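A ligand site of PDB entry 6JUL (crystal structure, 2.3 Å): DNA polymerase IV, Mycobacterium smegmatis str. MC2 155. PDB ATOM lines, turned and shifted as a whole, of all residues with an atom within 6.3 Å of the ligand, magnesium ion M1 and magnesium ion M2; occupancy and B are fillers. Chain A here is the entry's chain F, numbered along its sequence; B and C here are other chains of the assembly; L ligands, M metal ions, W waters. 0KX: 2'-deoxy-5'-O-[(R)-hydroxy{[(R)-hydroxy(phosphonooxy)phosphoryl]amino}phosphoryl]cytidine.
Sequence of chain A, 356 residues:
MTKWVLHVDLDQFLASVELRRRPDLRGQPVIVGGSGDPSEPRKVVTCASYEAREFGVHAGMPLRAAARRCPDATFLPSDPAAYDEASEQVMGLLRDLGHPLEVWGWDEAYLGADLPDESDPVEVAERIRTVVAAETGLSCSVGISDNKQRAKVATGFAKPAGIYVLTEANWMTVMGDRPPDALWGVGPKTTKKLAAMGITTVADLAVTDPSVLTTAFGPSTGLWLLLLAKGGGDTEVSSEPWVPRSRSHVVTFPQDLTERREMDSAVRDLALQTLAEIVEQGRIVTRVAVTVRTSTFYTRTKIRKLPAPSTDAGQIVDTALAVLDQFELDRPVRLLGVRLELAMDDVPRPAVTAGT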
ATOM      1  N   HIS A   7     -17.749   4.387  -4.749  1.00  0.00           N
ATOM      2  CA  HIS A   7     -17.774   2.939  -4.908  1.00  0.00           C
ATOM      3  C   HIS A   7     -16.378   2.372  -5.108  1.00  0.00           C
ATOM      4  O   HIS A   7     -15.710   2.690  -6.113  1.00  0.00           O
ATOM      5  CB  HIS A   7     -18.737   2.504  -6.043  1.00  0.00           C
ATOM      6  CG  HIS A   7     -18.818   1.035  -6.211  1.00  0.00           C
ATOM      7  ND1 HIS A   7     -18.233   0.382  -7.267  1.00  0.00           N
ATOM      8  CD2 HIS A   7     -19.270   0.081  -5.363  1.00  0.00           C
ATOM      9  CE1 HIS A   7     -18.401  -0.911  -7.118  1.00  0.00           C
ATOM     10  NE2 HIS A   7     -19.054  -1.133  -5.986  1.00  0.00           N
ATOM     11  N   ASP A   9     -14.015  -0.824  -5.860  1.00  0.00           N
ATOM     12  CA  ASP A   9     -14.055  -2.136  -6.410  1.00  0.00           C
ATOM     13  C   ASP A   9     -12.622  -2.750  -6.681  1.00  0.00           C
ATOM     14  O   ASP A   9     -11.898  -2.223  -7.451  1.00  0.00           O
ATOM     15  CB  ASP A   9     -14.982  -2.183  -7.607  1.00  0.00           C
ATOM     16  CG  ASP A   9     -15.148  -3.599  -8.195  1.00  0.00           C
ATOM     17  OD1 ASP A   9     -14.133  -4.128  -8.746  1.00  0.00           O
ATOM     18  OD2 ASP A   9     -16.253  -4.195  -8.094  1.00  0.00           O
ATOM     19  N   LEU A  10     -12.263  -3.846  -6.019  1.00  0.00           N
ATOM     20  CA  LEU A  10     -10.983  -4.533  -6.283  1.00  0.00           C
ATOM     21  C   LEU A  10     -10.801  -5.054  -7.729  1.00  0.00           C
ATOM     22  O   LEU A  10     -11.768  -5.642  -8.351  1.00  0.00           O
ATOM     23  CB  LEU A  10     -10.830  -5.672  -5.270  1.00  0.00           C
ATOM     24  CG  LEU A  10     -10.548  -4.974  -3.928  1.00  0.00           C
ATOM     25  CD1 LEU A  10     -10.901  -5.925  -2.829  1.00  0.00           C
ATOM     26  CD2 LEU A  10      -9.050  -4.558  -3.884  1.00  0.00           C
ATOM     27  N   ASP A  11      -9.651  -4.738  -8.298  1.00  0.00           N
ATOM     28  CA  ASP A  11      -9.295  -5.096  -9.680  1.00  0.00           C
ATOM     29  C   ASP A  11      -9.006  -6.553  -9.789  1.00  0.00           C
ATOM     30  O   ASP A  11      -8.173  -7.076  -9.024  1.00  0.00           O
ATOM     31  CB  ASP A  11      -8.131  -4.282 -10.238  1.00  0.00           C
ATOM     32  CG  ASP A  11      -8.462  -2.829 -10.412  1.00  0.00           C
ATOM     33  OD1 ASP A  11      -9.672  -2.382 -10.354  1.00  0.00           O
ATOM     34  OD2 ASP A  11      -7.536  -2.066 -10.565  1.00  0.00           O
ATOM     35  N   GLN A  12      -9.720  -7.225 -10.701  1.00  0.00           N
ATOM     36  CA  GLN A  12      -9.536  -8.675 -11.026  1.00  0.00           C
ATOM     37  C   GLN A  12      -9.256  -9.483  -9.713  1.00  0.00           C
ATOM     38  O   GLN A  12      -8.239 -10.146  -9.575  1.00  0.00           O
ATOM     39  CB  GLN A  12      -8.465  -8.858 -12.133  1.00  0.00           C
ATOM     40  CG  GLN A  12      -7.011  -8.547 -11.670  1.00  0.00           C
ATOM     41  CD  GLN A  12      -5.892  -8.771 -12.669  1.00  0.00           C
ATOM     42  OE1 GLN A  12      -5.968  -9.640 -13.499  1.00  0.00           O
ATOM     43  NE2 GLN A  12      -4.872  -7.967 -12.618  1.00  0.00           N
ATOM     44  N   PHE A  13     -10.160  -9.310  -8.740  1.00  0.00           N
ATOM     45  CA  PHE A  13      -9.913  -9.619  -7.363  1.00  0.00           C
ATOM     46  C   PHE A  13      -9.254 -11.020  -7.151  1.00  0.00           C
ATOM     47  O   PHE A  13      -8.170 -11.082  -6.550  1.00  0.00           O
ATOM     48  CB  PHE A  13     -11.174  -9.499  -6.573  1.00  0.00           C
ATOM     49  CG  PHE A  13     -11.008  -9.877  -5.119  1.00  0.00           C
ATOM     50  CD1 PHE A  13      -9.948  -9.334  -4.341  1.00  0.00           C
ATOM     51  CD2 PHE A  13     -11.902 -10.773  -4.486  1.00  0.00           C
ATOM     52  CE1 PHE A  13      -9.791  -9.708  -3.009  1.00  0.00           C
ATOM     53  CE2 PHE A  13     -11.700 -11.148  -3.142  1.00  0.00           C
ATOM     54  CZ  PHE A  13     -10.664 -10.597  -2.404  1.00  0.00           C
ATOM     55  N   LEU A  14      -9.837 -12.115  -7.620  1.00  0.00           N
ATOM     56  CA  LEU A  14      -9.276 -13.422  -7.184  1.00  0.00           C
ATOM     57  C   LEU A  14      -7.919 -13.618  -7.829  1.00  0.00           C
ATOM     58  O   LEU A  14      -6.964 -13.990  -7.196  1.00  0.00           O
ATOM     59  CB  LEU A  14     -10.209 -14.567  -7.494  1.00  0.00           C
ATOM     60  CG  LEU A  14     -11.470 -14.907  -6.654  1.00  0.00           C
ATOM     61  CD1 LEU A  14     -12.294 -13.834  -6.087  1.00  0.00           C
ATOM     62  CD2 LEU A  14     -12.391 -15.775  -7.517  1.00  0.00           C
ATOM     63  N   ALA A  15      -7.821 -13.294  -9.099  1.00  0.00           N
ATOM     64  CA  ALA A  15      -6.524 -13.340  -9.771  1.00  0.00           C
ATOM     65  C   ALA A  15      -5.447 -12.505  -9.055  1.00  0.00           C
ATOM     66  O   ALA A  15      -4.252 -12.960  -8.949  1.00  0.00           O
ATOM     67  CB  ALA A  15      -6.639 -12.929 -11.217  1.00  0.00           C
ATOM     68  N   VAL A  45     -15.120 -20.476 -15.167  1.00  0.00           N
ATOM     69  CA  VAL A  45     -14.245 -19.428 -14.731  1.00  0.00           C
ATOM     70  C   VAL A  45     -14.952 -18.519 -13.746  1.00  0.00           C
ATOM     71  O   VAL A  45     -16.091 -18.034 -13.950  1.00  0.00           O
ATOM     72  CB  VAL A  45     -13.713 -18.589 -15.890  1.00  0.00           C
ATOM     73  CG1 VAL A  45     -12.882 -17.391 -15.358  1.00  0.00           C
ATOM     74  CG2 VAL A  45     -12.893 -19.432 -16.900  1.00  0.00           C
ATOM     75  N   THR A  46     -14.236 -18.280 -12.664  1.00  0.00           N
ATOM     76  CA  THR A  46     -14.723 -17.361 -11.689  1.00  0.00           C
ATOM     77  C   THR A  46     -14.012 -15.966 -11.664  1.00  0.00           C
ATOM     78  O   THR A  46     -14.635 -14.980 -11.399  1.00  0.00           O
ATOM     79  CB  THR A  46     -14.806 -18.108 -10.385  1.00  0.00           C
ATOM     80  OG1 THR A  46     -15.799 -17.454  -9.686  1.00  0.00           O
ATOM     81  CG2 THR A  46     -13.545 -18.024  -9.632  1.00  0.00           C
ATOM     82  N   CYS A  47     -12.727 -15.898 -12.034  1.00  0.00           N
ATOM     83  CA  CYS A  47     -12.016 -14.712 -12.211  1.00  0.00           C
ATOM     84  C   CYS A  47     -10.875 -14.960 -13.170  1.00  0.00           C
ATOM     85  O   CYS A  47      -9.932 -15.715 -12.873  1.00  0.00           O
ATOM     86  CB  CYS A  47     -11.471 -14.188 -10.871  1.00  0.00           C
ATOM     87  SG  CYS A  47     -10.432 -12.704 -11.176  1.00  0.00           S
ATOM     88  N   ALA A  48     -10.930 -14.311 -14.299  1.00  0.00           N
ATOM     89  CA  ALA A  48      -9.828 -14.388 -15.263  1.00  0.00           C
ATOM     90  C   ALA A  48      -8.978 -13.161 -14.996  1.00  0.00           C
ATOM     91  O   ALA A  48      -9.540 -12.050 -14.723  1.00  0.00           O
ATOM     92  CB  ALA A  48     -10.400 -14.347 -16.658  1.00  0.00           C
ATOM     93  N   TYR A  50      -6.677  -9.988 -16.096  1.00  0.00           N
ATOM     94  CA  TYR A  50      -6.731  -9.152 -17.306  1.00  0.00           C
ATOM     95  C   TYR A  50      -6.109  -9.773 -18.540  1.00  0.00           C
ATOM     96  O   TYR A  50      -6.644  -9.558 -19.656  1.00  0.00           O
ATOM     97  CB  TYR A  50      -6.234  -7.745 -17.081  1.00  0.00           C
ATOM     98  CG  TYR A  50      -7.023  -6.968 -16.026  1.00  0.00           C
ATOM     99  CD1 TYR A  50      -8.347  -7.266 -15.759  1.00  0.00           C
ATOM    100  CD2 TYR A  50      -6.440  -5.915 -15.346  1.00  0.00           C
ATOM    101  CE1 TYR A  50      -9.122  -6.555 -14.832  1.00  0.00           C
ATOM    102  CE2 TYR A  50      -7.177  -5.122 -14.410  1.00  0.00           C
ATOM    103  CZ  TYR A  50      -8.528  -5.456 -14.135  1.00  0.00           C
ATOM    104  OH  TYR A  50      -9.292  -4.696 -13.240  1.00  0.00           O
ATOM    105  N   ARG A  53      -8.392 -12.080 -20.123  1.00  0.00           N
ATOM    106  CA  ARG A  53      -9.648 -11.457 -20.699  1.00  0.00           C
ATOM    107  C   ARG A  53      -9.291 -11.013 -22.114  1.00  0.00           C
ATOM    108  O   ARG A  53     -10.146 -10.917 -22.976  1.00  0.00           O
ATOM    109  CB  ARG A  53     -10.187 -10.263 -19.840  1.00  0.00           C
ATOM    110  CG  ARG A  53     -10.789 -10.703 -18.462  1.00  0.00           C
ATOM    111  CD  ARG A  53     -11.229  -9.584 -17.522  1.00  0.00           C
ATOM    112  NE  ARG A  53     -11.112  -9.930 -16.067  1.00  0.00           N
ATOM    113  CZ  ARG A  53     -11.743  -9.318 -15.040  1.00  0.00           C
ATOM    114  NH1 ARG A  53     -12.450  -8.235 -15.212  1.00  0.00           N
ATOM    115  NH2 ARG A  53     -11.532  -9.725 -13.785  1.00  0.00           N
ATOM    116  N   ALA A  59     -15.720 -14.232 -16.342  1.00  0.00           N
ATOM    117  CA  ALA A  59     -16.481 -14.912 -15.291  1.00  0.00           C
ATOM    118  C   ALA A  59     -17.696 -15.563 -15.908  1.00  0.00           C
ATOM    119  O   ALA A  59     -18.452 -14.865 -16.532  1.00  0.00           O
ATOM    120  CB  ALA A  59     -16.896 -13.902 -14.196  1.00  0.00           C
ATOM    121  N   GLY A  60     -17.909 -16.884 -15.688  1.00  0.00           N
ATOM    122  CA  GLY A  60     -19.161 -17.596 -16.046  1.00  0.00           C
ATOM    123  C   GLY A  60     -18.871 -18.475 -17.249  1.00  0.00           C
ATOM    124  O   GLY A  60     -19.616 -19.436 -17.560  1.00  0.00           O
ATOM    125  N   TRP A 106     -17.198  -9.931  -1.307  1.00  0.00           N
ATOM    126  CA  TRP A 106     -15.770  -9.959  -1.092  1.00  0.00           C
ATOM    127  C   TRP A 106     -15.162  -8.629  -1.526  1.00  0.00           C
ATOM    128  O   TRP A 106     -14.261  -8.184  -0.861  1.00  0.00           O
ATOM    129  CB  TRP A 106     -15.120 -11.037  -1.952  1.00  0.00           C
ATOM    130  CG  TRP A 106     -15.036 -12.426  -1.429  1.00  0.00           C
ATOM    131  CD1 TRP A 106     -14.828 -12.857  -0.101  1.00  0.00           C
ATOM    132  CD2 TRP A 106     -14.993 -13.612  -2.219  1.00  0.00           C
ATOM    133  NE1 TRP A 106     -14.731 -14.232  -0.041  1.00  0.00           N
ATOM    134  CE2 TRP A 106     -14.848 -14.724  -1.324  1.00  0.00           C
ATOM    135  CE3 TRP A 106     -15.172 -13.855  -3.595  1.00  0.00           C
ATOM    136  CZ2 TRP A 106     -14.789 -16.021  -1.767  1.00  0.00           C
ATOM    137  CZ3 TRP A 106     -15.152 -15.139  -4.043  1.00  0.00           C
ATOM    138  CH2 TRP A 106     -14.957 -16.218  -3.140  1.00  0.00           C
ATOM    139  N   ASP A 107     -15.687  -8.025  -2.607  1.00  0.00           N
ATOM    140  CA  ASP A 107     -14.876  -7.271  -3.582  1.00  0.00           C
ATOM    141  C   ASP A 107     -15.166  -5.807  -3.532  1.00  0.00           C
ATOM    142  O   ASP A 107     -14.383  -4.987  -4.096  1.00  0.00           O
ATOM    143  CB  ASP A 107     -15.324  -7.732  -5.033  1.00  0.00           C
ATOM    144  CG  ASP A 107     -14.672  -6.912  -6.179  1.00  0.00           C
ATOM    145  OD1 ASP A 107     -13.511  -7.050  -6.520  1.00  0.00           O
ATOM    146  OD2 ASP A 107     -15.280  -6.037  -6.836  1.00  0.00           O
ATOM    147  N   GLU A 108     -16.353  -5.473  -2.992  1.00  0.00           N
ATOM    148  CA  GLU A 108     -16.844  -4.110  -3.092  1.00  0.00           C
ATOM    149  C   GLU A 108     -17.518  -3.450  -1.852  1.00  0.00           C
ATOM    150  O   GLU A 108     -17.963  -4.105  -0.917  1.00  0.00           O
ATOM    151  CB  GLU A 108     -17.793  -3.953  -4.275  1.00  0.00           C
ATOM    152  CG  GLU A 108     -18.554  -5.142  -4.694  1.00  0.00           C
ATOM    153  CD  GLU A 108     -19.356  -4.715  -5.868  1.00  0.00           C
ATOM    154  OE1 GLU A 108     -20.154  -3.752  -5.680  1.00  0.00           O
ATOM    155  OE2 GLU A 108     -19.120  -5.239  -7.002  1.00  0.00           O
ATOM    156  N   LYS A 152     -21.492   3.123  -9.248  1.00  0.00           N
ATOM    157  CA  LYS A 152     -21.252   1.796  -9.679  1.00  0.00           C
ATOM    158  C   LYS A 152     -20.954   1.910 -11.161  1.00  0.00           C
ATOM    159  O   LYS A 152     -19.922   1.428 -11.608  1.00  0.00           O
ATOM    160  CB  LYS A 152     -22.488   0.937  -9.259  1.00  0.00           C
ATOM    161  CG  LYS A 152     -22.399  -0.502  -9.572  1.00  0.00           C
ATOM    162  CD  LYS A 152     -21.451  -1.145  -8.586  1.00  0.00           C
ATOM    163  CE  LYS A 152     -21.825  -2.604  -8.239  1.00  0.00           C
ATOM    164  NZ  LYS A 152     -20.645  -3.502  -8.485  1.00  0.00           N
ATOM    165  N   LYS A 159     -12.198   1.639 -14.329  1.00  0.00           N
ATOM    166  CA  LYS A 159     -11.427   0.394 -14.586  1.00  0.00           C
ATOM    167  C   LYS A 159     -10.410   0.579 -15.754  1.00  0.00           C
ATOM    168  O   LYS A 159     -10.787   1.130 -16.816  1.00  0.00           O
ATOM    169  CB  LYS A 159     -12.350  -0.811 -14.954  1.00  0.00           C
ATOM    170  CG  LYS A 159     -13.129  -1.442 -13.773  1.00  0.00           C
ATOM    171  CD  LYS A 159     -12.224  -2.135 -12.772  1.00  0.00           C
ATOM    172  CE  LYS A 159     -13.054  -2.416 -11.514  1.00  0.00           C
ATOM    173  NZ  LYS A 159     -12.293  -3.098 -10.384  1.00  0.00           N
ATOM    174  P    DC B  18     -22.125  -6.213 -10.464  1.00  0.00           P
ATOM    175  OP1  DC B  18     -21.671  -4.854 -10.210  1.00  0.00           O
ATOM    176  OP2  DC B  18     -21.973  -6.842 -11.789  1.00  0.00           O
ATOM    177  O5'  DC B  18     -21.508  -7.254  -9.435  1.00  0.00           O
ATOM    178  C5'  DC B  18     -21.652  -7.085  -7.987  1.00  0.00           C
ATOM    179  C4'  DC B  18     -20.965  -8.241  -7.290  1.00  0.00           C
ATOM    180  O4'  DC B  18     -21.760  -9.426  -7.506  1.00  0.00           O
ATOM    181  C3'  DC B  18     -19.581  -8.543  -7.880  1.00  0.00           C
ATOM    182  O3'  DC B  18     -18.499  -7.925  -7.158  1.00  0.00           O
ATOM    183  C2'  DC B  18     -19.498 -10.045  -7.831  1.00  0.00           C
ATOM    184  C1'  DC B  18     -20.932 -10.544  -7.662  1.00  0.00           C
ATOM    185  N1   DC B  18     -21.493 -11.379  -8.738  1.00  0.00           N
ATOM    186  C2   DC B  18     -21.675 -12.724  -8.457  1.00  0.00           C
ATOM    187  O2   DC B  18     -21.331 -13.142  -7.353  1.00  0.00           O
ATOM    188  N3   DC B  18     -22.294 -13.523  -9.363  1.00  0.00           N
ATOM    189  C4   DC B  18     -22.641 -13.024 -10.561  1.00  0.00           C
ATOM    190  N4   DC B  18     -23.199 -13.857 -11.459  1.00  0.00           N
ATOM    191  C5   DC B  18     -22.436 -11.651 -10.893  1.00  0.00           C
ATOM    192  C6   DC B  18     -21.856 -10.866  -9.960  1.00  0.00           C
ATOM    193  P    DG C   4     -23.858 -24.070 -15.076  1.00  0.00           P
ATOM    194  OP1  DG C   4     -24.241 -25.483 -15.049  1.00  0.00           O
ATOM    195  OP2  DG C   4     -24.824 -23.020 -14.812  1.00  0.00           O
ATOM    196  O5'  DG C   4     -22.681 -23.791 -14.043  1.00  0.00           O
ATOM    197  C5'  DG C   4     -21.576 -24.664 -13.841  1.00  0.00           C
ATOM    198  C4'  DG C   4     -21.129 -24.521 -12.403  1.00  0.00           C
ATOM    199  O4'  DG C   4     -20.591 -23.194 -12.209  1.00  0.00           O
ATOM    200  C3'  DG C   4     -22.245 -24.672 -11.383  1.00  0.00           C
ATOM    201  O3'  DG C   4     -21.749 -25.383 -10.231  1.00  0.00           O
ATOM    202  C2'  DG C   4     -22.671 -23.221 -11.122  1.00  0.00           C
ATOM    203  C1'  DG C   4     -21.370 -22.449 -11.308  1.00  0.00           C
ATOM    204  N9   DG C   4     -21.484 -21.130 -11.898  1.00  0.00           N
ATOM    205  C8   DG C   4     -22.062 -20.863 -13.115  1.00  0.00           C
ATOM    206  N7   DG C   4     -21.997 -19.614 -13.455  1.00  0.00           N
ATOM    207  C5   DG C   4     -21.297 -19.017 -12.415  1.00  0.00           C
ATOM    208  C6   DG C   4     -20.890 -17.670 -12.257  1.00  0.00           C
ATOM    209  O6   DG C   4     -21.092 -16.707 -13.000  1.00  0.00           O
ATOM    210  N1   DG C   4     -20.219 -17.485 -11.059  1.00  0.00           N
ATOM    211  C2   DG C   4     -19.939 -18.465 -10.137  1.00  0.00           C
ATOM    212  N2   DG C   4     -19.237 -18.060  -9.057  1.00  0.00           N
ATOM    213  N3   DG C   4     -20.254 -19.747 -10.315  1.00  0.00           N
ATOM    214  C4   DG C   4     -20.944 -19.943 -11.463  1.00  0.00           C
ATOM    215  P    DG C   5     -22.736 -25.638  -8.982  1.00  0.00           P
ATOM    216  OP1  DG C   5     -22.362 -26.879  -8.326  1.00  0.00           O
ATOM    217  OP2  DG C   5     -24.177 -25.540  -9.448  1.00  0.00           O
ATOM    218  O5'  DG C   5     -22.428 -24.335  -8.101  1.00  0.00           O
ATOM    219  C5'  DG C   5     -21.212 -24.083  -7.404  1.00  0.00           C
ATOM    220  C4'  DG C   5     -21.468 -22.904  -6.489  1.00  0.00           C
ATOM    221  O4'  DG C   5     -21.555 -21.712  -7.294  1.00  0.00           O
ATOM    222  C3'  DG C   5     -22.742 -22.965  -5.648  1.00  0.00           C
ATOM    223  O3'  DG C   5     -22.372 -22.607  -4.323  1.00  0.00           O
ATOM    224  C2'  DG C   5     -23.677 -21.945  -6.291  1.00  0.00           C
ATOM    225  C1'  DG C   5     -22.671 -20.944  -6.830  1.00  0.00           C
ATOM    226  N9   DG C   5     -23.129 -20.088  -7.928  1.00  0.00           N
ATOM    227  C8   DG C   5     -23.861 -20.477  -9.012  1.00  0.00           C
ATOM    228  N7   DG C   5     -24.113 -19.494  -9.840  1.00  0.00           N
ATOM    229  C5   DG C   5     -23.482 -18.394  -9.267  1.00  0.00           C
ATOM    230  C6   DG C   5     -23.365 -17.035  -9.734  1.00  0.00           C
ATOM    231  O6   DG C   5     -23.846 -16.527 -10.744  1.00  0.00           O
ATOM    232  N1   DG C   5     -22.633 -16.262  -8.843  1.00  0.00           N
ATOM    233  C2   DG C   5     -22.066 -16.708  -7.675  1.00  0.00           C
ATOM    234  N2   DG C   5     -21.364 -15.809  -6.977  1.00  0.00           N
ATOM    235  N3   DG C   5     -22.106 -17.968  -7.274  1.00  0.00           N
ATOM    236  C4   DG C   5     -22.846 -18.753  -8.107  1.00  0.00           C
HETATM  237  PG  0KX L   1     -12.910  -6.395 -12.111  1.00  0.00           P
HETATM  238  O1G 0KX L   1     -13.661  -5.950 -10.786  1.00  0.00           O
HETATM  239  O2G 0KX L   1     -13.532  -6.367 -13.473  1.00  0.00           O
HETATM  240  O3G 0KX L   1     -11.572  -5.647 -12.084  1.00  0.00           O
HETATM  241  PB  0KX L   1     -13.332  -8.904 -10.714  1.00  0.00           P
HETATM  242  O1B 0KX L   1     -13.062  -8.180  -9.375  1.00  0.00           O
HETATM  243  O2B 0KX L   1     -12.809 -10.322 -10.727  1.00  0.00           O
HETATM  244  O3B 0KX L   1     -12.645  -7.975 -11.817  1.00  0.00           O
HETATM  245  PA  0KX L   1     -16.206  -8.358 -10.051  1.00  0.00           P
HETATM  246  O1A 0KX L   1     -17.290  -8.168 -11.042  1.00  0.00           O
HETATM  247  O2A 0KX L   1     -15.755  -7.216  -9.113  1.00  0.00           O
HETATM  248  N3A 0KX L   1     -14.928  -8.773 -11.032  1.00  0.00           N
HETATM  249  O5' 0KX L   1     -16.532  -9.644  -9.174  1.00  0.00           O
HETATM  250  C5' 0KX L   1     -15.645  -9.853  -8.035  1.00  0.00           C
HETATM  251  C4' 0KX L   1     -15.445 -11.288  -7.618  1.00  0.00           C
HETATM  252  O4' 0KX L   1     -16.740 -11.858  -7.530  1.00  0.00           O
HETATM  253  C3' 0KX L   1     -14.701 -12.062  -8.670  1.00  0.00           C
HETATM  254  O3' 0KX L   1     -13.279 -11.893  -8.717  1.00  0.00           O
HETATM  255  C2' 0KX L   1     -15.174 -13.468  -8.444  1.00  0.00           C
HETATM  256  C1' 0KX L   1     -16.632 -13.210  -7.978  1.00  0.00           C
HETATM  257  N1  0KX L   1     -17.538 -13.370  -9.148  1.00  0.00           N
HETATM  258  C2  0KX L   1     -18.094 -14.607  -9.423  1.00  0.00           C
HETATM  259  N3  0KX L   1     -18.925 -14.728 -10.463  1.00  0.00           N
HETATM  260  C4  0KX L   1     -19.247 -13.737 -11.326  1.00  0.00           C
HETATM  261  C5  0KX L   1     -18.733 -12.452 -11.130  1.00  0.00           C
HETATM  262  C6  0KX L   1     -17.850 -12.329 -10.030  1.00  0.00           C
HETATM  263  O2  0KX L   1     -17.823 -15.593  -8.743  1.00  0.00           O
HETATM  264  N4  0KX L   1     -20.070 -14.035 -12.355  1.00  0.00           N
HETATM  265 MG    MG M   1     -17.282  -6.181  -7.799  1.00  0.00          MG
HETATM  266 MG    MG M   2     -13.876  -6.295  -8.619  1.00  0.00          MG
HETATM  267  O   HOH W   1     -14.422 -12.165 -12.422  1.00  0.00           O
HETATM  268  O   HOH W   2     -16.151  -4.750 -11.191  1.00  0.00           O
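CA of Asp 11 touches O3G of the ligand (3.4 Å). CD1 of Leu 14 touches O3' of the ligand, at 3.4 Å. CB of Ala 59 touches N4 of the ligand, at 3.7 Å. DG 5 of chain C touches the ligand. Hydrophobic or aromatic side chains that line the ligand: Phe 13, Leu 14, Tyr 50 and Ala 59. 16 residues have an atom within 4 Å of the ligand: Asp 9, Leu 10, Asp 11, Gln 12, Phe 13, Leu 14, Thr 46, Cys 47, Tyr 50, Arg 53, Ala 59, Asp 107, Lys 159, DC 18 of chain B, DG 4 of chain C and DG 5 of chain C.
Within 4 Å of magnesium ion M1: Asp 9, Asp 107, Glu 108 and DC 18 of chain B. The nearest printed residue that does not touch magnesium ion M1 is Lys 152 (4.4 Å).
O2B of the ligand sits at hydrogen-bond distance from SG of Cys 47. An oxygen (O3G) of the ligand is in hydrogen-bond range of the side-chain hydroxyl (OH) of Tyr 50. O6 of DG 4 of chain C sits at hydrogen-bond distance from a nitrogen (N4) of the ligand, at 2.9 Å. An oxygen (O2B) of the ligand sits at hydrogen-bond distance from the backbone NH of Phe 13. An oxygen (O2) of the ligand is in hydrogen-bond range of the side-chain hydroxyl of Thr 46, 2.9 Å away. O3G of the ligand is in salt-bridge range of NZ of Lys 159 (3.1 Å). An oxygen (O3G) of the ligand is in hydrogen-bond range of the backbone NH (N) of Gln 12, at 2.8 Å. N4 of the ligand is in hydrogen-bond range of N4 of DC 18 of chain B. An oxygen (O2G) of the ligand lies within salt-bridge range of the guanidinium group (NH1) of Arg 53, 2.8 Å away.
The backbone carbonyl oxygen of Leu 10 lies close to the side-chain amino group of Lys 159, at 3.3 Å. NZ of Lys 152 lies within salt-bridge range of OE1 of Glu 108 (2.9 Å). The side-chain amino group of Lys 159 lies within hydrogen-bond range of the backbone carbonyl oxygen of Asp 9 (3.1 Å). The side-chain sulfur (SG) of Cys 47 sits close to the backbone carbonyl oxygen (O) of Gln 12 (3.7 Å). The backbone NH (N) of Leu 14 sits at hydrogen-bond distance from the side-chain sulfur (SG) of Cys 47. OE1 of Gln 12 sits at hydrogen-bond distance from N of Tyr 50, 2.7 Å away. O2 of DC 18 of chain B sits close to N2 of DG 5 of chain C. The side-chain carboxylate (OE1) of Glu 108 is in hydrogen-bond range of a ring nitrogen (NE2) of His 7.
Magnesium ion M1 is bound by the side-chain carboxylate of Glu 108, O3' of DC 18 of chain B, the side-chain carboxylate of Asp 107, the side-chain carboxylate of Asp 9 and an oxygen (O2A) of the ligand.
Water W1 bridges an oxygen (O2B) of the ligand and the backbone carbonyl oxygen (O) of Thr 46.
NZ of Lys 159 touches magnesium ion M2 (3.98 Å). Four residues have an atom within 4 Å of magnesium ion M2: Asp 9, Leu 10, Asp 107 and Lys 159.
Magnesium ion M2 is bound by O2A of the ligand (2.2 Å), OD1 of Asp 9 (2.2 Å), O1B of the ligand (2.2 Å), O1G of the ligand (2.2 Å), O of Leu 10 (2.2 Å), OD1 of Asp 107 (2.3 Å) and OD2 of Asp 107 (2.3 Å).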
